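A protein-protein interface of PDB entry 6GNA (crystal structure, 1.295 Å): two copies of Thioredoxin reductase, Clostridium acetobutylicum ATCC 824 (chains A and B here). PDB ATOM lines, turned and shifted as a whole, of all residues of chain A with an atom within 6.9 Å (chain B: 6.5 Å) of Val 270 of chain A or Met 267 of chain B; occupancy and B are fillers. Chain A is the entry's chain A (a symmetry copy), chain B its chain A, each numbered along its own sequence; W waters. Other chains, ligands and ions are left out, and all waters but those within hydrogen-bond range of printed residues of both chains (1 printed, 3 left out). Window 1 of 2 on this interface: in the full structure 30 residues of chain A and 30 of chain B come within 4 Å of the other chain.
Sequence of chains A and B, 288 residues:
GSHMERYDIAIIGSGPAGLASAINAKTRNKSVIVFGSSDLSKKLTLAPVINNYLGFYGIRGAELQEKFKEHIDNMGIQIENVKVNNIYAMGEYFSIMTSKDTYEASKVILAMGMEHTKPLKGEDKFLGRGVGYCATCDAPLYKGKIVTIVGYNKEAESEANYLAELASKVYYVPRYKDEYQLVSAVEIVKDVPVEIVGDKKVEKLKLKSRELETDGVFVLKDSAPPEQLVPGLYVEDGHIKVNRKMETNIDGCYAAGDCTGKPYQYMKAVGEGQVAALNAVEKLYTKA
ND2 of Asn 52 of chain B is in hydrogen-bond range of OD1 of Asn 24 of chain A, 3.4 Å away.
O of Leu 54 of chain B is in hydrogen-bond range of OH of Tyr 53 of chain A, at 3.0 Å.
OE1 of Gln 274 of chain A lies close to N of Met 267 of chain B (3.3 Å).
N of Lys 268 of chain B is in hydrogen-bond range of OE1 of Gln 274 of chain A (2.9 Å).
ND2 of Asn 52 of chain B lies within hydrogen-bond range of OE1 of Gln 265 of chain B, at 2.7 Å.
The side-chain amino group of Lys 268 of chain B is in salt-bridge range of the side-chain carboxylate of Glu 272 of chain B (3.2 Å).
The side-chain amide nitrogen (ND2) of Asn 24 of chain A lies within hydrogen-bond range of the backbone carbonyl oxygen (O) of Ala 20 of chain A.
The side-chain amide oxygen (OD1) of Asn 24 of chain A is in hydrogen-bond range of the side-chain amide nitrogen (NE2) of Gln 274 of chain A.
The side-chain amino group of Lys 268 of chain A is in hydrogen-bond range of the backbone carbonyl oxygen of Gly 257 of chain A (2.8 Å).
NZ of Lys 268 of chain A is in salt-bridge range of OE1 of Glu 272 of chain A, at 3.2 Å.
Among the printed residues, merely in contact across the chains: Gln 274 of chain A with Gln 265 of chain B (3.1 Å), Gly 271 of chain A with Met 267 of chain B (3.3 Å), Met 267 of chain A with Gly 271 of chain B (3.3 Å), Asn 24 of chain A with Met 267 of chain B (3.4 Å), Gln 274 of chain A with Asn 52 of chain B (3.5 Å), Phe 68 of chain A with Leu 54 of chain B (3.5 Å), Ala 20 of chain A with Met 267 of chain B (3.6 Å), Met 267 of chain A with Val 270 of chain B (3.7 Å), Val 270 of chain A with Met 267 of chain B (3.7 Å), Ile 23 of chain A with Asn 52 of chain B (3.8 Å), Gly 271 of chain A with Lys 268 of chain B (3.8 Å), Lys 268 of chain A with Gly 271 of chain B (3.8 Å), Val 275 of chain A with Lys 268 of chain B (3.8 Å), Ile 23 of chain A with Leu 54 of chain B (3.8 Å), Pro 16 of chain A with Leu 54 of chain B (3.9 Å), Val 270 of chain A with Leu 54 of chain B (3.9 Å) and Leu 19 of chain A with Leu 54 of chain B (3.95 Å).
Of chain B, only Leu 54 (3.9 Å) and Met 267 (3.7 Å) come within 4 Å of Val 270 of chain A.
Met 267 of chain B touches just these residues of chain A: Ala 20, Asn 24, Val 270, Gly 271 and Gln 274.
Of the printed residues of chain B, Tyr 53 of chain A touches Leu 54.
Printed residues of chain A within 4 Å of Val 270 of chain B: Met 267 (3.7 Å).
Of the printed residues of chain B, Leu 19 of chain A touches Leu 54 (3.95 Å).
Of the printed residues of chain A, Gly 271 of chain B touches Met 267 and Lys 268.
Ser 21 of chain A touches none of the printed residues of chain B.
Gly 15 of chain A touches none of the printed residues of chain B.
The nearest printed residue of chain B that does not touch Phe 68 of chain A is Tyr 53 of chain B (6.7 Å).
Hydrophobic or aromatic side chains of chain B within 4 Å of the printed part of chain A: Leu 54, Met 267 and Val 270.
Printed residues of chain A that touch a printed residue of chain B: Pro 16, Leu 19, Ala 20, Ile 23, Asn 24, Tyr 53, Phe 68, Met 267, Lys 268, Val 270, Gly 271, Gln 274 and Val 275.
Hydrophobic or aromatic side chains of chain A that line the printed part of chain B: Leu 19, Ala 20, Ile 23, Tyr 53, Phe 68, Met 267, Val 270 and Val 275.
Met 267 of chain A touches Val 270 of chain B, and with the chains exchanged Val 270 of chain A touches Met 267 of chain B.
Met 267 of chain A touches Gly 271 of chain B, and with the chains exchanged Gly 271 of chain A touches Met 267 of chain B.
Lys 268 of chain A touches Gly 271 of chain B, and with the chains exchanged Gly 271 of chain A touches Lys 268 of chain B.
9 positions are printed for both chains.
Water W1 bridges the side-chain amide oxygen of Asn 24 of chain A and the side-chain amide nitrogen of Asn 52 of chain B.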
ATOM      1  N   GLY A  15      20.432  24.467  16.638  1.00  0.00           N
ATOM      2  CA  GLY A  15      19.089  24.088  16.289  1.00  0.00           C
ATOM      3  C   GLY A  15      18.957  23.889  14.797  1.00  0.00           C
ATOM      4  O   GLY A  15      19.939  23.904  14.049  1.00  0.00           O
ATOM      5  N   PRO A  16      17.709  23.757  14.326  1.00  0.00           N
ATOM      6  CA  PRO A  16      17.452  23.584  12.892  1.00  0.00           C
ATOM      7  C   PRO A  16      18.268  24.505  11.995  1.00  0.00           C
ATOM      8  O   PRO A  16      18.859  24.060  11.003  1.00  0.00           O
ATOM      9  CB  PRO A  16      15.943  23.847  12.792  1.00  0.00           C
ATOM     10  CG  PRO A  16      15.415  23.394  14.134  1.00  0.00           C
ATOM     11  CD  PRO A  16      16.488  23.686  15.139  1.00  0.00           C
ATOM     12  N   ALA A  17      18.285  25.813  12.282  1.00  0.00           N
ATOM     13  CA  ALA A  17      19.006  26.756  11.429  1.00  0.00           C
ATOM     14  C   ALA A  17      20.511  26.476  11.426  1.00  0.00           C
ATOM     15  O   ALA A  17      21.147  26.427  10.366  1.00  0.00           O
ATOM     16  CB  ALA A  17      18.698  28.199  11.840  1.00  0.00           C
ATOM     17  N   GLY A  18      21.109  26.347  12.597  1.00  0.00           N
ATOM     18  CA  GLY A  18      22.544  26.122  12.643  1.00  0.00           C
ATOM     19  C   GLY A  18      22.971  24.793  12.041  1.00  0.00           C
ATOM     20  O   GLY A  18      24.008  24.711  11.377  1.00  0.00           O
ATOM     21  N   LEU A  19      22.192  23.730  12.267  1.00  0.00           N
ATOM     22  CA  LEU A  19      22.523  22.445  11.660  1.00  0.00           C
ATOM     23  C   LEU A  19      22.364  22.497  10.148  1.00  0.00           C
ATOM     24  O   LEU A  19      23.182  21.925   9.418  1.00  0.00           O
ATOM     25  CB  LEU A  19      21.659  21.331  12.257  1.00  0.00           C
ATOM     26  CG  LEU A  19      21.795  21.201  13.776  1.00  0.00           C
ATOM     27  CD1 LEU A  19      21.044  20.004  14.269  1.00  0.00           C
ATOM     28  CD2 LEU A  19      23.266  21.161  14.249  1.00  0.00           C
ATOM     29  N   ALA A  20      21.335  23.193   9.658  1.00  0.00           N
ATOM     30  CA  ALA A  20      21.197  23.368   8.219  1.00  0.00           C
ATOM     31  C   ALA A  20      22.399  24.109   7.655  1.00  0.00           C
ATOM     32  O   ALA A  20      22.904  23.769   6.582  1.00  0.00           O
ATOM     33  CB  ALA A  20      19.899  24.112   7.911  1.00  0.00           C
ATOM     34  N   SER A  21      22.876  25.139   8.355  1.00  0.00           N
ATOM     35  CA  SER A  21      24.096  25.800   7.913  1.00  0.00           C
ATOM     36  C   SER A  21      25.270  24.826   7.884  1.00  0.00           C
ATOM     37  O   SER A  21      26.021  24.757   6.903  1.00  0.00           O
ATOM     38  CB  SER A  21      24.413  26.964   8.845  1.00  0.00           C
ATOM     39  OG  SER A  21      23.500  28.036   8.708  1.00  0.00           O
ATOM     40  N   ILE A  23      25.535  21.489   7.625  1.00  0.00           N
ATOM     41  CA  ILE A  23      25.586  20.443   6.599  1.00  0.00           C
ATOM     42  C   ILE A  23      25.837  21.030   5.218  1.00  0.00           C
ATOM     43  O   ILE A  23      26.282  20.310   4.315  1.00  0.00           O
ATOM     44  CB  ILE A  23      24.345  19.537   6.613  1.00  0.00           C
ATOM     45  CG1 ILE A  23      23.080  20.282   6.191  1.00  0.00           C
ATOM     46  CG2 ILE A  23      24.159  18.909   7.984  1.00  0.00           C
ATOM     47  CD1 ILE A  23      21.877  19.355   6.017  1.00  0.00           C
ATOM     48  N   ASN A  24      25.549  22.312   5.026  1.00  0.00           N
ATOM     49  CA  ASN A  24      25.818  22.969   3.754  1.00  0.00           C
ATOM     50  C   ASN A  24      27.195  23.604   3.699  1.00  0.00           C
ATOM     51  O   ASN A  24      27.724  23.815   2.606  1.00  0.00           O
ATOM     52  CB  ASN A  24      24.739  24.015   3.467  1.00  0.00           C
ATOM     53  CG  ASN A  24      23.478  23.389   2.954  1.00  0.00           C
ATOM     54  OD1 ASN A  24      23.380  23.080   1.754  1.00  0.00           O
ATOM     55  ND2 ASN A  24      22.519  23.143   3.850  1.00  0.00           N
ATOM     56  N   TYR A  53       6.700  19.771   8.474  1.00  0.00           N
ATOM     57  CA  TYR A  53       8.061  19.578   7.990  1.00  0.00           C
ATOM     58  C   TYR A  53       7.997  18.537   6.874  1.00  0.00           C
ATOM     59  O   TYR A  53       7.831  17.338   7.134  1.00  0.00           O
ATOM     60  CB  TYR A  53       8.998  19.179   9.124  1.00  0.00           C
ATOM     61  CG  TYR A  53      10.458  19.262   8.752  1.00  0.00           C
ATOM     62  CD1 TYR A  53      11.153  20.428   8.886  1.00  0.00           C
ATOM     63  CD2 TYR A  53      11.155  18.132   8.330  1.00  0.00           C
ATOM     64  CE1 TYR A  53      12.493  20.515   8.547  1.00  0.00           C
ATOM     65  CE2 TYR A  53      12.513  18.199   7.982  1.00  0.00           C
ATOM     66  CZ  TYR A  53      13.175  19.424   8.105  1.00  0.00           C
ATOM     67  OH  TYR A  53      14.513  19.647   7.805  1.00  0.00           O
ATOM     68  N   PHE A  68      18.002  14.557  13.018  1.00  0.00           N
ATOM     69  CA  PHE A  68      18.977  15.620  12.800  1.00  0.00           C
ATOM     70  C   PHE A  68      20.327  15.242  13.405  1.00  0.00           C
ATOM     71  O   PHE A  68      21.383  15.507  12.811  1.00  0.00           O
ATOM     72  CB  PHE A  68      18.466  16.930  13.424  1.00  0.00           C
ATOM     73  CG  PHE A  68      17.303  17.598  12.691  1.00  0.00           C
ATOM     74  CD1 PHE A  68      16.789  17.112  11.503  1.00  0.00           C
ATOM     75  CD2 PHE A  68      16.756  18.784  13.210  1.00  0.00           C
ATOM     76  CE1 PHE A  68      15.732  17.763  10.859  1.00  0.00           C
ATOM     77  CE2 PHE A  68      15.703  19.425  12.576  1.00  0.00           C
ATOM     78  CZ  PHE A  68      15.194  18.917  11.399  1.00  0.00           C
ATOM     79  N   ALA A 256      20.193  33.371  10.585  1.00  0.00           N
ATOM     80  CA  ALA A 256      19.262  32.383  10.060  1.00  0.00           C
ATOM     81  C   ALA A 256      18.390  31.829  11.171  1.00  0.00           C
ATOM     82  O   ALA A 256      18.858  31.595  12.293  1.00  0.00           O
ATOM     83  CB  ALA A 256      20.041  31.233   9.412  1.00  0.00           C
ATOM     84  N   GLY A 257      17.124  31.577  10.831  1.00  0.00           N
ATOM     85  CA  GLY A 257      16.181  30.950  11.718  1.00  0.00           C
ATOM     86  C   GLY A 257      15.339  31.914  12.518  1.00  0.00           C
ATOM     87  O   GLY A 257      15.078  33.043  12.078  1.00  0.00           O
ATOM     88  N   GLN A 265       9.215  28.822  12.311  1.00  0.00           N
ATOM     89  CA  GLN A 265       8.952  27.466  11.835  1.00  0.00           C
ATOM     90  C   GLN A 265      10.245  26.772  11.411  1.00  0.00           C
ATOM     91  O   GLN A 265      11.224  27.428  11.056  1.00  0.00           O
ATOM     92  CB  GLN A 265       8.000  27.496  10.632  1.00  0.00           C
ATOM     93  CG  GLN A 265       6.619  28.096  10.872  1.00  0.00           C
ATOM     94  CD  GLN A 265       5.695  27.183  11.652  1.00  0.00           C
ATOM     95  OE1 GLN A 265       4.715  26.672  11.112  1.00  0.00           O
ATOM     96  NE2 GLN A 265       6.002  26.968  12.924  1.00  0.00           N
ATOM     97  N   TYR A 266      10.238  25.443  11.439  1.00  0.00           N
ATOM     98  CA  TYR A 266      11.407  24.658  11.040  1.00  0.00           C
ATOM     99  C   TYR A 266      11.868  24.807   9.587  1.00  0.00           C
ATOM    100  O   TYR A 266      13.060  24.969   9.338  1.00  0.00           O
ATOM    101  CB  TYR A 266      11.135  23.164  11.262  1.00  0.00           C
ATOM    102  CG  TYR A 266      10.787  22.770  12.677  1.00  0.00           C
ATOM    103  CD1 TYR A 266      11.683  22.969  13.717  1.00  0.00           C
ATOM    104  CD2 TYR A 266       9.571  22.166  12.966  1.00  0.00           C
ATOM    105  CE1 TYR A 266      11.368  22.597  15.011  1.00  0.00           C
ATOM    106  CE2 TYR A 266       9.249  21.791  14.254  1.00  0.00           C
ATOM    107  CZ  TYR A 266      10.148  22.008  15.272  1.00  0.00           C
ATOM    108  OH  TYR A 266       9.826  21.635  16.555  1.00  0.00           O
ATOM    109  N   MET A 267      10.944  24.764   8.629  1.00  0.00           N
ATOM    110  CA  MET A 267      11.339  24.855   7.221  1.00  0.00           C
ATOM    111  C   MET A 267      11.961  26.210   6.894  1.00  0.00           C
ATOM    112  O   MET A 267      12.981  26.277   6.209  1.00  0.00           O
ATOM    113  CB  MET A 267      10.178  24.487   6.298  1.00  0.00           C
ATOM    114  CG  MET A 267       9.772  23.028   6.470  1.00  0.00           C
ATOM    115  SD  MET A 267       9.028  22.258   5.021  1.00  0.00           S
ATOM    116  CE  MET A 267       7.543  23.247   4.855  1.00  0.00           C
ATOM    117  N   LYS A 268      11.361  27.286   7.390  1.00  0.00           N
ATOM    118  CA  LYS A 268      11.967  28.602   7.231  1.00  0.00           C
ATOM    119  C   LYS A 268      13.383  28.597   7.794  1.00  0.00           C
ATOM    120  O   LYS A 268      14.330  29.044   7.140  1.00  0.00           O
ATOM    121  CB  LYS A 268      11.127  29.672   7.924  1.00  0.00           C
ATOM    122  CG  LYS A 268      11.812  31.053   7.881  1.00  0.00           C
ATOM    123  CD  LYS A 268      11.068  32.186   8.572  1.00  0.00           C
ATOM    124  CE  LYS A 268      11.575  32.494   9.996  1.00  0.00           C
ATOM    125  NZ  LYS A 268      12.952  33.054  10.217  1.00  0.00           N
ATOM    126  N   ALA A 269      13.550  28.050   8.999  1.00  0.00           N
ATOM    127  CA  ALA A 269      14.861  28.056   9.632  1.00  0.00           C
ATOM    128  C   ALA A 269      15.898  27.284   8.824  1.00  0.00           C
ATOM    129  O   ALA A 269      17.027  27.751   8.646  1.00  0.00           O
ATOM    130  CB  ALA A 269      14.745  27.487  11.049  1.00  0.00           C
ATOM    131  N   VAL A 270      15.561  26.079   8.344  1.00  0.00           N
ATOM    132  CA  VAL A 270      16.580  25.305   7.634  1.00  0.00           C
ATOM    133  C   VAL A 270      16.906  25.935   6.292  1.00  0.00           C
ATOM    134  O   VAL A 270      18.054  25.900   5.826  1.00  0.00           O
ATOM    135  CB  VAL A 270      16.223  23.804   7.532  1.00  0.00           C
ATOM    136  CG1 VAL A 270      16.097  23.194   8.913  1.00  0.00           C
ATOM    137  CG2 VAL A 270      14.949  23.523   6.732  1.00  0.00           C
ATOM    138  N   GLY A 271      15.903  26.508   5.643  1.00  0.00           N
ATOM    139  CA  GLY A 271      16.166  27.227   4.402  1.00  0.00           C
ATOM    140  C   GLY A 271      17.109  28.402   4.592  1.00  0.00           C
ATOM    141  O   GLY A 271      18.042  28.607   3.814  1.00  0.00           O
ATOM    142  N   GLU A 272      16.851  29.204   5.613  1.00  0.00           N
ATOM    143  CA  GLU A 272      17.739  30.323   5.931  1.00  0.00           C
ATOM    144  C   GLU A 272      19.147  29.852   6.293  1.00  0.00           C
ATOM    145  O   GLU A 272      20.144  30.458   5.880  1.00  0.00           O
ATOM    146  CB  GLU A 272      17.134  31.148   7.069  1.00  0.00           C
ATOM    147  CG  GLU A 272      15.903  31.917   6.619  1.00  0.00           C
ATOM    148  CD  GLU A 272      15.348  32.874   7.646  1.00  0.00           C
ATOM    149  OE1 GLU A 272      15.804  32.915   8.808  1.00  0.00           O
ATOM    150  OE2 GLU A 272      14.431  33.638   7.278  1.00  0.00           O
ATOM    151  N   GLY A 273      19.266  28.784   7.076  1.00  0.00           N
ATOM    152  CA  GLY A 273      20.600  28.292   7.392  1.00  0.00           C
ATOM    153  C   GLY A 273      21.357  27.873   6.144  1.00  0.00           C
ATOM    154  O   GLY A 273      22.556  28.157   6.002  1.00  0.00           O
ATOM    155  N   GLN A 274      20.671  27.206   5.223  1.00  0.00           N
ATOM    156  CA  GLN A 274      21.306  26.807   3.980  1.00  0.00           C
ATOM    157  C   GLN A 274      21.789  28.012   3.188  1.00  0.00           C
ATOM    158  O   GLN A 274      22.923  28.033   2.701  1.00  0.00           O
ATOM    159  CB  GLN A 274      20.319  25.999   3.147  1.00  0.00           C
ATOM    160  CG  GLN A 274      20.839  25.686   1.798  1.00  0.00           C
ATOM    161  CD  GLN A 274      20.006  24.637   1.150  1.00  0.00           C
ATOM    162  OE1 GLN A 274      18.819  24.843   0.879  1.00  0.00           O
ATOM    163  NE2 GLN A 274      20.598  23.454   0.961  1.00  0.00           N
ATOM    164  N   VAL A 275      20.921  29.013   3.020  1.00  0.00           N
ATOM    165  CA  VAL A 275      21.283  30.197   2.240  1.00  0.00           C
ATOM    166  C   VAL A 275      22.473  30.915   2.866  1.00  0.00           C
ATOM    167  O   VAL A 275      23.415  31.311   2.168  1.00  0.00           O
ATOM    168  CB  VAL A 275      20.068  31.124   2.091  1.00  0.00           C
ATOM    169  CG1 VAL A 275      20.489  32.433   1.411  1.00  0.00           C
ATOM    170  CG2 VAL A 275      18.976  30.440   1.281  1.00  0.00           C
ATOM    171  N   ASN B  52      22.159  17.152   1.741  1.00  0.00           N
ATOM    172  CA  ASN B  52      21.972  18.470   2.328  1.00  0.00           C
ATOM    173  C   ASN B  52      20.506  18.788   2.564  1.00  0.00           C
ATOM    174  O   ASN B  52      20.136  19.968   2.594  1.00  0.00           O
ATOM    175  CB  ASN B  52      22.646  19.541   1.473  1.00  0.00           C
ATOM    176  CG  ASN B  52      21.966  19.732   0.143  1.00  0.00           C
ATOM    177  OD1 ASN B  52      21.107  18.950  -0.243  1.00  0.00           O
ATOM    178  ND2 ASN B  52      22.324  20.812  -0.556  1.00  0.00           N
ATOM    179  N   TYR B  53      19.666  17.782   2.718  1.00  0.00           N
ATOM    180  CA  TYR B  53      18.305  17.962   3.205  1.00  0.00           C
ATOM    181  C   TYR B  53      18.255  17.393   4.622  1.00  0.00           C
ATOM    182  O   TYR B  53      18.250  16.170   4.814  1.00  0.00           O
ATOM    183  CB  TYR B  53      17.294  17.314   2.267  1.00  0.00           C
ATOM    184  CG  TYR B  53      15.869  17.722   2.546  1.00  0.00           C
ATOM    185  CD1 TYR B  53      15.335  18.845   1.986  1.00  0.00           C
ATOM    186  CD2 TYR B  53      15.036  16.925   3.328  1.00  0.00           C
ATOM    187  CE1 TYR B  53      14.028  19.229   2.236  1.00  0.00           C
ATOM    188  CE2 TYR B  53      13.708  17.296   3.595  1.00  0.00           C
ATOM    189  CZ  TYR B  53      13.216  18.473   3.024  1.00  0.00           C
ATOM    190  OH  TYR B  53      11.929  18.968   3.189  1.00  0.00           O
ATOM    191  N   LEU B  54      18.180  18.299   5.595  1.00  0.00           N
ATOM    192  CA  LEU B  54      18.432  17.965   6.992  1.00  0.00           C
ATOM    193  C   LEU B  54      17.407  16.958   7.501  1.00  0.00           C
ATOM    194  O   LEU B  54      16.191  17.179   7.419  1.00  0.00           O
ATOM    195  CB  LEU B  54      18.401  19.230   7.839  1.00  0.00           C
ATOM    196  CG  LEU B  54      18.768  19.035   9.319  1.00  0.00           C
ATOM    197  CD1 LEU B  54      20.209  18.552   9.521  1.00  0.00           C
ATOM    198  CD2 LEU B  54      18.510  20.316  10.094  1.00  0.00           C
ATOM    199  N   GLN B 265      18.307  25.105  -4.174  1.00  0.00           N
ATOM    200  CA  GLN B 265      18.395  23.987  -3.237  1.00  0.00           C
ATOM    201  C   GLN B 265      17.032  23.674  -2.624  1.00  0.00           C
ATOM    202  O   GLN B 265      16.160  24.540  -2.553  1.00  0.00           O
ATOM    203  CB  GLN B 265      19.373  24.317  -2.101  1.00  0.00           C
ATOM    204  CG  GLN B 265      20.816  24.598  -2.505  1.00  0.00           C
ATOM    205  CD  GLN B 265      21.588  23.349  -2.882  1.00  0.00           C
ATOM    206  OE1 GLN B 265      22.502  22.938  -2.170  1.00  0.00           O
ATOM    207  NE2 GLN B 265      21.222  22.736  -3.999  1.00  0.00           N
ATOM    208  N   TYR B 266      16.858  22.435  -2.173  1.00  0.00           N
ATOM    209  CA  TYR B 266      15.603  22.012  -1.549  1.00  0.00           C
ATOM    210  C   TYR B 266      15.203  22.734  -0.259  1.00  0.00           C
ATOM    211  O   TYR B 266      14.051  23.135  -0.115  1.00  0.00           O
ATOM    212  CB  TYR B 266      15.664  20.517  -1.213  1.00  0.00           C
ATOM    213  CG  TYR B 266      15.919  19.597  -2.383  1.00  0.00           C
ATOM    214  CD1 TYR B 266      15.032  19.529  -3.448  1.00  0.00           C
ATOM    215  CD2 TYR B 266      17.034  18.771  -2.405  1.00  0.00           C
ATOM    216  CE1 TYR B 266      15.262  18.679  -4.513  1.00  0.00           C
ATOM    217  CE2 TYR B 266      17.270  17.918  -3.464  1.00  0.00           C
ATOM    218  CZ  TYR B 266      16.383  17.876  -4.515  1.00  0.00           C
ATOM    219  OH  TYR B 266      16.619  17.027  -5.569  1.00  0.00           O
ATOM    220  N   MET B 267      16.137  22.913   0.674  1.00  0.00           N
ATOM    221  CA  MET B 267      15.793  23.556   1.945  1.00  0.00           C
ATOM    222  C   MET B 267      15.370  25.009   1.748  1.00  0.00           C
ATOM    223  O   MET B 267      14.386  25.455   2.337  1.00  0.00           O
ATOM    224  CB  MET B 267      16.917  23.390   2.967  1.00  0.00           C
ATOM    225  CG  MET B 267      17.116  21.926   3.342  1.00  0.00           C
ATOM    226  SD  MET B 267      17.786  21.634   4.989  1.00  0.00           S
ATOM    227  CE  MET B 267      19.395  22.405   4.826  1.00  0.00           C
ATOM    228  N   LYS B 268      16.097  25.743   0.915  1.00  0.00           N
ATOM    229  CA  LYS B 268      15.680  27.098   0.575  1.00  0.00           C
ATOM    230  C   LYS B 268      14.263  27.083   0.016  1.00  0.00           C
ATOM    231  O   LYS B 268      13.402  27.860   0.441  1.00  0.00           O
ATOM    232  CB  LYS B 268      16.640  27.723  -0.434  1.00  0.00           C
ATOM    233  CG  LYS B 268      16.150  29.107  -0.908  1.00  0.00           C
ATOM    234  CD  LYS B 268      17.023  29.804  -1.940  1.00  0.00           C
ATOM    235  CE  LYS B 268      16.527  29.647  -3.392  1.00  0.00           C
ATOM    236  NZ  LYS B 268      15.233  30.271  -3.834  1.00  0.00           N
ATOM    237  N   ALA B 269      13.992  26.169  -0.917  1.00  0.00           N
ATOM    238  CA  ALA B 269      12.679  26.124  -1.542  1.00  0.00           C
ATOM    239  C   ALA B 269      11.567  25.843  -0.538  1.00  0.00           C
ATOM    240  O   ALA B 269      10.517  26.491  -0.568  1.00  0.00           O
ATOM    241  CB  ALA B 269      12.681  25.075  -2.658  1.00  0.00           C
ATOM    242  N   VAL B 270      11.750  24.856   0.351  1.00  0.00           N
ATOM    243  CA  VAL B 270      10.653  24.535   1.266  1.00  0.00           C
ATOM    244  C   VAL B 270      10.451  25.642   2.283  1.00  0.00           C
ATOM    245  O   VAL B 270       9.320  25.933   2.701  1.00  0.00           O
ATOM    246  CB  VAL B 270      10.806  23.137   1.909  1.00  0.00           C
ATOM    247  CG1 VAL B 270      10.814  22.060   0.842  1.00  0.00           C
ATOM    248  CG2 VAL B 270      12.050  22.992   2.788  1.00  0.00           C
ATOM    249  N   GLY B 271      11.538  26.268   2.708  1.00  0.00           N
ATOM    250  CA  GLY B 271      11.406  27.414   3.601  1.00  0.00           C
ATOM    251  C   GLY B 271      10.627  28.559   2.978  1.00  0.00           C
ATOM    252  O   GLY B 271       9.751  29.154   3.607  1.00  0.00           O
ATOM    253  N   GLU B 272      10.966  28.897   1.745  1.00  0.00           N
ATOM    254  CA  GLU B 272      10.229  29.937   1.024  1.00  0.00           C
ATOM    255  C   GLU B 272       8.762  29.563   0.819  1.00  0.00           C
ATOM    256  O   GLU B 272       7.868  30.406   0.963  1.00  0.00           O
ATOM    257  CB  GLU B 272      10.913  30.208  -0.319  1.00  0.00           C
ATOM    258  CG  GLU B 272      12.248  30.913  -0.143  1.00  0.00           C
ATOM    259  CD  GLU B 272      12.901  31.352  -1.431  1.00  0.00           C
ATOM    260  OE1 GLU B 272      12.425  31.036  -2.542  1.00  0.00           O
ATOM    261  OE2 GLU B 272      13.922  32.066  -1.339  1.00  0.00           O
HETATM  262  O   HOH W   1      25.411  21.951  -0.065  1.00  0.00           O
